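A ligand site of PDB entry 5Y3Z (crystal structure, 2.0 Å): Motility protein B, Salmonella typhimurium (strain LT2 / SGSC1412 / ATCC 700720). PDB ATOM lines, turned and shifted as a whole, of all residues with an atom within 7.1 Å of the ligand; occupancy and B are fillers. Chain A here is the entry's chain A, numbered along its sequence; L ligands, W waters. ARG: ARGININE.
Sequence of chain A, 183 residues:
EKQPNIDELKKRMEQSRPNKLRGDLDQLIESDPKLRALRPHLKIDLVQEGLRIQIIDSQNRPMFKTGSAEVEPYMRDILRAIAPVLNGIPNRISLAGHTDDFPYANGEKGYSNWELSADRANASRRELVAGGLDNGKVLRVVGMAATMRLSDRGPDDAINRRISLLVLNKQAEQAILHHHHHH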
ATOM      1  N   PHE A  64      27.847 -19.909 -23.527  1.00  0.00           N
ATOM      2  CA  PHE A  64      26.615 -20.333 -22.879  1.00  0.00           C
ATOM      3  C   PHE A  64      25.523 -19.284 -23.044  1.00  0.00           C
ATOM      4  O   PHE A  64      25.794 -18.087 -22.987  1.00  0.00           O
ATOM      5  CB  PHE A  64      26.838 -20.604 -21.383  1.00  0.00           C
ATOM      6  CG  PHE A  64      27.564 -21.884 -21.092  1.00  0.00           C
ATOM      7  CD1 PHE A  64      26.892 -23.099 -21.114  1.00  0.00           C
ATOM      8  CD2 PHE A  64      28.912 -21.879 -20.775  1.00  0.00           C
ATOM      9  CE1 PHE A  64      27.546 -24.282 -20.835  1.00  0.00           C
ATOM     10  CE2 PHE A  64      29.575 -23.065 -20.494  1.00  0.00           C
ATOM     11  CZ  PHE A  64      28.899 -24.258 -20.520  1.00  0.00           C
ATOM     12  N   LYS A  65      24.283 -19.735 -23.247  1.00  0.00           N
ATOM     13  CA  LYS A  65      23.149 -18.831 -23.197  1.00  0.00           C
ATOM     14  C   LYS A  65      23.018 -18.320 -21.768  1.00  0.00           C
ATOM     15  O   LYS A  65      23.412 -18.996 -20.821  1.00  0.00           O
ATOM     16  CB  LYS A  65      21.861 -19.525 -23.636  1.00  0.00           C
ATOM     17  CG  LYS A  65      21.813 -19.887 -25.113  1.00  0.00           C
ATOM     18  CD  LYS A  65      20.508 -20.594 -25.460  1.00  0.00           C
ATOM     19  CE  LYS A  65      20.432 -20.947 -26.940  1.00  0.00           C
ATOM     20  NZ  LYS A  65      19.138 -21.596 -27.306  1.00  0.00           N
ATOM     21  N   THR A  66      22.464 -17.116 -21.607  1.00  0.00           N
ATOM     22  CA  THR A  66      22.327 -16.532 -20.283  1.00  0.00           C
ATOM     23  C   THR A  66      21.446 -17.413 -19.390  1.00  0.00           C
ATOM     24  O   THR A  66      20.340 -17.808 -19.766  1.00  0.00           O
ATOM     25  CB  THR A  66      21.748 -15.098 -20.346  1.00  0.00           C
ATOM     26  OG1 THR A  66      21.529 -14.604 -19.022  1.00  0.00           O
ATOM     27  CG2 THR A  66      20.442 -15.059 -21.136  1.00  0.00           C
ATOM     28  N   GLY A  67      21.973 -17.748 -18.207  1.00  0.00           N
ATOM     29  CA  GLY A  67      21.266 -18.594 -17.257  1.00  0.00           C
ATOM     30  C   GLY A  67      21.252 -20.060 -17.617  1.00  0.00           C
ATOM     31  O   GLY A  67      20.605 -20.861 -16.945  1.00  0.00           O
ATOM     32  N   SER A  68      21.980 -20.440 -18.660  1.00  0.00           N
ATOM     33  CA  SER A  68      21.969 -21.820 -19.146  1.00  0.00           C
ATOM     34  C   SER A  68      23.280 -22.548 -18.899  1.00  0.00           C
ATOM     35  O   SER A  68      24.369 -21.979 -19.042  1.00  0.00           O
ATOM     36  CB  SER A  68      21.637 -21.853 -20.639  1.00  0.00           C
ATOM     37  OG  SER A  68      21.631 -23.181 -21.123  1.00  0.00           O
ATOM     38  N   ALA A  69      23.173 -23.822 -18.525  1.00  0.00           N
ATOM     39  CA  ALA A  69      24.335 -24.680 -18.347  1.00  0.00           C
ATOM     40  C   ALA A  69      24.403 -25.702 -19.479  1.00  0.00           C
ATOM     41  O   ALA A  69      25.168 -26.657 -19.424  1.00  0.00           O
ATOM     42  CB  ALA A  69      24.293 -25.373 -17.001  1.00  0.00           C
ATOM     43  N   HIS A  98      32.107 -20.855 -14.950  1.00  0.00           N
ATOM     44  CA  HIS A  98      32.094 -19.418 -14.709  1.00  0.00           C
ATOM     45  C   HIS A  98      30.780 -18.785 -15.174  1.00  0.00           C
ATOM     46  O   HIS A  98      30.106 -19.316 -16.056  1.00  0.00           O
ATOM     47  CB  HIS A  98      33.268 -18.737 -15.415  1.00  0.00           C
ATOM     48  CG  HIS A  98      34.590 -19.392 -15.149  1.00  0.00           C
ATOM     49  ND1 HIS A  98      35.389 -19.058 -14.082  1.00  0.00           N
ATOM     50  CD2 HIS A  98      35.260 -20.369 -15.819  1.00  0.00           C
ATOM     51  CE1 HIS A  98      36.490 -19.786 -14.104  1.00  0.00           C
ATOM     52  NE2 HIS A  98      36.436 -20.594 -15.148  1.00  0.00           N
ATOM     53  N   THR A  99      30.433 -17.650 -14.569  1.00  0.00           N
ATOM     54  CA  THR A  99      29.240 -16.909 -14.963  1.00  0.00           C
ATOM     55  C   THR A  99      29.570 -15.430 -15.163  1.00  0.00           C
ATOM     56  O   THR A  99      30.631 -14.960 -14.743  1.00  0.00           O
ATOM     57  CB  THR A  99      28.122 -17.013 -13.905  1.00  0.00           C
ATOM     58  OG1 THR A  99      28.541 -16.358 -12.697  1.00  0.00           O
ATOM     59  CG2 THR A  99      27.788 -18.466 -13.608  1.00  0.00           C
ATOM     60  N   ASP A 100      28.664 -14.685 -15.813  1.00  0.00           N
ATOM     61  CA  ASP A 100      28.757 -13.231 -15.791  1.00  0.00           C
ATOM     62  C   ASP A 100      28.202 -12.760 -14.456  1.00  0.00           C
ATOM     63  O   ASP A 100      27.735 -13.570 -13.648  1.00  0.00           O
ATOM     64  CB  ASP A 100      28.032 -12.597 -16.988  1.00  0.00           C
ATOM     65  CG  ASP A 100      26.543 -12.944 -17.053  1.00  0.00           C
ATOM     66  OD1 ASP A 100      25.896 -13.102 -16.004  1.00  0.00           O
ATOM     67  OD2 ASP A 100      26.019 -13.039 -18.182  1.00  0.00           O
ATOM     68  N   ASP A 101      28.238 -11.452 -14.180  1.00  0.00           N
ATOM     69  CA  ASP A 101      27.795 -11.001 -12.865  1.00  0.00           C
ATOM     70  C   ASP A 101      26.335 -10.567 -12.848  1.00  0.00           C
ATOM     71  O   ASP A 101      25.910  -9.832 -11.957  1.00  0.00           O
ATOM     72  CB  ASP A 101      28.698  -9.867 -12.355  1.00  0.00           C
ATOM     73  CG  ASP A 101      28.802  -8.703 -13.331  1.00  0.00           C
ATOM     74  OD1 ASP A 101      27.851  -8.472 -14.098  1.00  0.00           O
ATOM     75  OD2 ASP A 101      29.845  -8.020 -13.314  1.00  0.00           O
ATOM     76  N   PHE A 102      25.573 -11.019 -13.831  1.00  0.00           N
ATOM     77  CA  PHE A 102      24.121 -10.820 -13.804  1.00  0.00           C
ATOM     78  C   PHE A 102      23.547 -11.724 -12.723  1.00  0.00           C
ATOM     79  O   PHE A 102      23.640 -12.952 -12.811  1.00  0.00           O
ATOM     80  CB  PHE A 102      23.468 -11.107 -15.153  1.00  0.00           C
ATOM     81  CG  PHE A 102      22.111 -10.460 -15.329  1.00  0.00           C
ATOM     82  CD1 PHE A 102      21.028 -10.862 -14.553  1.00  0.00           C
ATOM     83  CD2 PHE A 102      21.925  -9.457 -16.257  1.00  0.00           C
ATOM     84  CE1 PHE A 102      19.788 -10.273 -14.710  1.00  0.00           C
ATOM     85  CE2 PHE A 102      20.679  -8.855 -16.417  1.00  0.00           C
ATOM     86  CZ  PHE A 102      19.612  -9.274 -15.647  1.00  0.00           C
ATOM     87  N   PRO A 103      22.945 -11.122 -11.689  1.00  0.00           N
ATOM     88  CA  PRO A 103      22.484 -11.867 -10.505  1.00  0.00           C
ATOM     89  C   PRO A 103      21.116 -12.506 -10.685  1.00  0.00           C
ATOM     90  O   PRO A 103      20.379 -12.170 -11.618  1.00  0.00           O
ATOM     91  CB  PRO A 103      22.432 -10.785  -9.433  1.00  0.00           C
ATOM     92  CG  PRO A 103      22.042  -9.559 -10.190  1.00  0.00           C
ATOM     93  CD  PRO A 103      22.682  -9.680 -11.558  1.00  0.00           C
ATOM     94  N   TYR A 104      20.781 -13.434  -9.796  1.00  0.00           N
ATOM     95  CA  TYR A 104      19.427 -13.966  -9.719  1.00  0.00           C
ATOM     96  C   TYR A 104      18.641 -13.125  -8.718  1.00  0.00           C
ATOM     97  O   TYR A 104      19.230 -12.351  -7.976  1.00  0.00           O
ATOM     98  CB  TYR A 104      19.446 -15.441  -9.342  1.00  0.00           C
ATOM     99  CG  TYR A 104      19.862 -16.339 -10.491  1.00  0.00           C
ATOM    100  CD1 TYR A 104      21.194 -16.604 -10.739  1.00  0.00           C
ATOM    101  CD2 TYR A 104      18.911 -16.898 -11.337  1.00  0.00           C
ATOM    102  CE1 TYR A 104      21.585 -17.416 -11.803  1.00  0.00           C
ATOM    103  CE2 TYR A 104      19.279 -17.712 -12.392  1.00  0.00           C
ATOM    104  CZ  TYR A 104      20.622 -17.967 -12.620  1.00  0.00           C
ATOM    105  OH  TYR A 104      20.993 -18.771 -13.676  1.00  0.00           O
ATOM    106  N   SER A 112      21.740 -19.605  -7.501  1.00  0.00           N
ATOM    107  CA  SER A 112      22.581 -18.455  -7.812  1.00  0.00           C
ATOM    108  C   SER A 112      23.632 -18.784  -8.851  1.00  0.00           C
ATOM    109  O   SER A 112      23.602 -19.846  -9.475  1.00  0.00           O
ATOM    110  CB  SER A 112      23.247 -17.928  -6.544  1.00  0.00           C
ATOM    111  OG  SER A 112      24.182 -18.875  -6.041  1.00  0.00           O
ATOM    112  N   ASN A 113      24.569 -17.851  -9.047  1.00  0.00           N
ATOM    113  CA  ASN A 113      25.665 -18.063  -9.982  1.00  0.00           C
ATOM    114  C   ASN A 113      26.610 -19.156  -9.514  1.00  0.00           C
ATOM    115  O   ASN A 113      27.379 -19.704 -10.302  1.00  0.00           O
ATOM    116  CB  ASN A 113      26.439 -16.757 -10.192  1.00  0.00           C
ATOM    117  CG  ASN A 113      25.758 -15.843 -11.200  1.00  0.00           C
ATOM    118  OD1 ASN A 113      25.149 -16.299 -12.151  1.00  0.00           O
ATOM    119  ND2 ASN A 113      25.874 -14.538 -10.979  1.00  0.00           N
ATOM    120  N   LEU A 116      24.911 -22.245 -10.792  1.00  0.00           N
ATOM    121  CA  LEU A 116      24.989 -22.209 -12.247  1.00  0.00           C
ATOM    122  C   LEU A 116      26.390 -22.527 -12.765  1.00  0.00           C
ATOM    123  O   LEU A 116      26.551 -23.288 -13.722  1.00  0.00           O
ATOM    124  CB  LEU A 116      24.537 -20.854 -12.775  1.00  0.00           C
ATOM    125  CG  LEU A 116      24.655 -20.649 -14.287  1.00  0.00           C
ATOM    126  CD1 LEU A 116      23.880 -21.713 -15.044  1.00  0.00           C
ATOM    127  CD2 LEU A 116      24.162 -19.269 -14.670  1.00  0.00           C
ATOM    128  N   ARG A 120      27.705 -25.736 -14.940  1.00  0.00           N
ATOM    129  CA  ARG A 120      28.440 -25.585 -16.195  1.00  0.00           C
ATOM    130  C   ARG A 120      29.715 -26.421 -16.186  1.00  0.00           C
ATOM    131  O   ARG A 120      30.110 -26.974 -17.213  1.00  0.00           O
ATOM    132  CB  ARG A 120      28.764 -24.111 -16.446  1.00  0.00           C
ATOM    133  CG  ARG A 120      27.579 -23.326 -16.959  1.00  0.00           C
ATOM    134  CD  ARG A 120      27.886 -21.848 -17.150  1.00  0.00           C
ATOM    135  NE  ARG A 120      26.756 -21.161 -17.764  1.00  0.00           N
ATOM    136  CZ  ARG A 120      26.511 -19.865 -17.638  1.00  0.00           C
ATOM    137  NH1 ARG A 120      27.323 -19.096 -16.919  1.00  0.00           N
ATOM    138  NH2 ARG A 120      25.447 -19.325 -18.232  1.00  0.00           N
ATOM    139  N   ALA A 145      31.494 -18.910 -10.048  1.00  0.00           N
ATOM    140  CA  ALA A 145      30.575 -17.813 -10.291  1.00  0.00           C
ATOM    141  C   ALA A 145      31.228 -16.761 -11.198  1.00  0.00           C
ATOM    142  O   ALA A 145      31.741 -17.092 -12.265  1.00  0.00           O
ATOM    143  CB  ALA A 145      30.118 -17.176  -8.978  1.00  0.00           C
ATOM    144  N   ALA A 146      31.225 -15.512 -10.762  1.00  0.00           N
ATOM    145  CA  ALA A 146      31.799 -14.426 -11.549  1.00  0.00           C
ATOM    146  C   ALA A 146      33.099 -13.892 -10.939  1.00  0.00           C
ATOM    147  O   ALA A 146      33.526 -12.782 -11.252  1.00  0.00           O
ATOM    148  CB  ALA A 146      30.795 -13.299 -11.711  1.00  0.00           C
ATOM    149  N   ASP A 157      30.485  -8.229 -20.403  1.00  0.00           N
ATOM    150  CA  ASP A 157      30.601  -9.182 -19.296  1.00  0.00           C
ATOM    151  C   ASP A 157      30.107 -10.573 -19.671  1.00  0.00           C
ATOM    152  O   ASP A 157      30.417 -11.549 -18.994  1.00  0.00           O
ATOM    153  CB  ASP A 157      29.835  -8.658 -18.087  1.00  0.00           C
ATOM    154  CG  ASP A 157      30.108  -9.461 -16.831  1.00  0.00           C
ATOM    155  OD1 ASP A 157      31.291  -9.759 -16.565  1.00  0.00           O
ATOM    156  OD2 ASP A 157      29.149  -9.798 -16.119  1.00  0.00           O
ATOM    157  N   ALA A 158      29.329 -10.650 -20.750  1.00  0.00           N
ATOM    158  CA  ALA A 158      28.722 -11.915 -21.176  1.00  0.00           C
ATOM    159  C   ALA A 158      29.769 -12.941 -21.608  1.00  0.00           C
ATOM    160  O   ALA A 158      29.484 -14.141 -21.645  1.00  0.00           O
ATOM    161  CB  ALA A 158      27.743 -11.655 -22.316  1.00  0.00           C
ATOM    162  N   ASN A 160      32.127 -13.962 -19.996  1.00  0.00           N
ATOM    163  CA  ASN A 160      32.532 -14.748 -18.826  1.00  0.00           C
ATOM    164  C   ASN A 160      31.710 -16.036 -18.683  1.00  0.00           C
ATOM    165  O   ASN A 160      32.059 -16.912 -17.887  1.00  0.00           O
ATOM    166  CB  ASN A 160      32.409 -13.910 -17.554  1.00  0.00           C
ATOM    167  CG  ASN A 160      33.326 -12.710 -17.574  1.00  0.00           C
ATOM    168  OD1 ASN A 160      34.551 -12.848 -17.495  1.00  0.00           O
ATOM    169  ND2 ASN A 160      32.745 -11.526 -17.675  1.00  0.00           N
ATOM    170  N   ARG A 161      30.622 -16.131 -19.444  1.00  0.00           N
ATOM    171  CA  ARG A 161      29.822 -17.345 -19.465  1.00  0.00           C
ATOM    172  C   ARG A 161      30.600 -18.476 -20.132  1.00  0.00           C
ATOM    173  O   ARG A 161      30.581 -18.617 -21.350  1.00  0.00           O
ATOM    174  CB  ARG A 161      28.501 -17.101 -20.200  1.00  0.00           C
ATOM    175  CG  ARG A 161      27.332 -16.823 -19.272  1.00  0.00           C
ATOM    176  CD  ARG A 161      26.472 -15.678 -19.772  1.00  0.00           C
ATOM    177  NE  ARG A 161      26.042 -15.843 -21.157  1.00  0.00           N
ATOM    178  CZ  ARG A 161      25.442 -14.891 -21.861  1.00  0.00           C
ATOM    179  NH1 ARG A 161      25.200 -13.714 -21.307  1.00  0.00           N
ATOM    180  NH2 ARG A 161      25.083 -15.115 -23.119  1.00  0.00           N
ATOM    181  N   ARG A 162      31.291 -19.273 -19.326  1.00  0.00           N
ATOM    182  CA  ARG A 162      32.249 -20.221 -19.859  1.00  0.00           C
ATOM    183  C   ARG A 162      32.666 -21.306 -18.881  1.00  0.00           C
ATOM    184  O   ARG A 162      32.266 -21.308 -17.719  1.00  0.00           O
ATOM    185  CB  ARG A 162      33.509 -19.467 -20.307  1.00  0.00           C
ATOM    186  CG  ARG A 162      34.382 -19.026 -19.141  1.00  0.00           C
ATOM    187  CD  ARG A 162      35.288 -17.864 -19.511  1.00  0.00           C
ATOM    188  NE  ARG A 162      36.351 -17.664 -18.535  1.00  0.00           N
ATOM    189  CZ  ARG A 162      36.214 -16.962 -17.415  1.00  0.00           C
ATOM    190  NH1 ARG A 162      35.051 -16.386 -17.127  1.00  0.00           N
ATOM    191  NH2 ARG A 162      37.240 -16.835 -16.581  1.00  0.00           N
HETATM  192  N   ARG L   1      24.917 -14.745 -14.509  1.00  0.00           N
HETATM  193  CA  ARG L   1      24.123 -15.710 -15.284  1.00  0.00           C
HETATM  194  C   ARG L   1      24.969 -16.389 -16.349  1.00  0.00           C
HETATM  195  O   ARG L   1      24.452 -17.059 -17.236  1.00  0.00           O
HETATM  196  CB  ARG L   1      22.921 -15.024 -15.923  1.00  0.00           C
HETATM  197  CG  ARG L   1      21.772 -14.770 -14.969  1.00  0.00           C
HETATM  198  CD  ARG L   1      20.608 -14.097 -15.685  1.00  0.00           C
HETATM  199  NE  ARG L   1      20.061 -14.932 -16.750  1.00  0.00           N
HETATM  200  CZ  ARG L   1      19.027 -15.753 -16.600  1.00  0.00           C
HETATM  201  NH1 ARG L   1      18.598 -16.475 -17.635  1.00  0.00           N
HETATM  202  NH2 ARG L   1      18.425 -15.855 -15.425  1.00  0.00           N
HETATM  203  OXT ARG L   1      26.200 -16.304 -16.338  1.00  0.00           O
HETATM  204  O   HOH W   1      18.261 -13.491 -13.299  1.00  0.00           O
HETATM  205  O   HOH W   2      16.914 -18.561 -16.205  1.00  0.00           O
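OG1 of Thr 99 sits close to OD1 of Asn 113, at 3.4 Å. The guanidinium group of Arg 161 is in salt-bridge range of the side-chain carboxylate of Asp 100. The side-chain amide nitrogen (ND2) of Asn 113 lies within hydrogen-bond range of the backbone carbonyl oxygen (O) of Phe 102 (3.3 Å). O of Asp 100 is in hydrogen-bond range of ND2 of Asn 113 (3.4 Å). The backbone NH (N) of Ala 146 lies within hydrogen-bond range of the side-chain hydroxyl (OG1) of Thr 99 (3.4 Å). OD1 of Asp 100 sits at hydrogen-bond distance from N of Phe 102. The backbone carbonyl oxygen of Lys 65 lies within hydrogen-bond range of the guanidinium group of Arg 120 (3.3 Å). NE of Arg 120 is in hydrogen-bond range of O of Ser 68 (2.8 Å).
A nitrogen (N) of the ligand is in hydrogen-bond range of the backbone carbonyl oxygen (O) of Phe 102, at 2.8 Å. The guanidinium group (NH2) of Arg 120 is in salt-bridge range of an oxygen (O) of the ligand (2.7 Å). A nitrogen (N) of the ligand sits at hydrogen-bond distance from the backbone carbonyl oxygen (O) of Asp 100, at 3.2 Å. NE of the ligand lies within hydrogen-bond range of OG1 of Thr 66 (2.7 Å). The side-chain amide oxygen (OD1) of Asn 113 sits at hydrogen-bond distance from a nitrogen (N) of the ligand, at 2.8 Å. O of Thr 66 sits at hydrogen-bond distance from NH1 of the ligand (3.1 Å). A nitrogen (N) of the ligand lies within salt-bridge range of the side-chain carboxylate (OD1) of Asp 100 (2.4 Å). The backbone NH (N) of Asp 100 sits at hydrogen-bond distance from an oxygen (OXT) of the ligand (3.0 Å). The backbone NH (N) of Gly 67 sits at hydrogen-bond distance from an oxygen (O) of the ligand, at 2.8 Å.
Thr 99 touches the ligand. Tyr 104 touches the ligand. Leu 116 touches the ligand. Arg 161 touches the ligand (CG to OXT, 3.2 Å). Hydrophobic or aromatic side chains that line the ligand: Phe 102, Tyr 104 and Leu 116.
Water W1 lies within hydrogen-bond range of O of Pro 103 and NH2 of the ligand.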
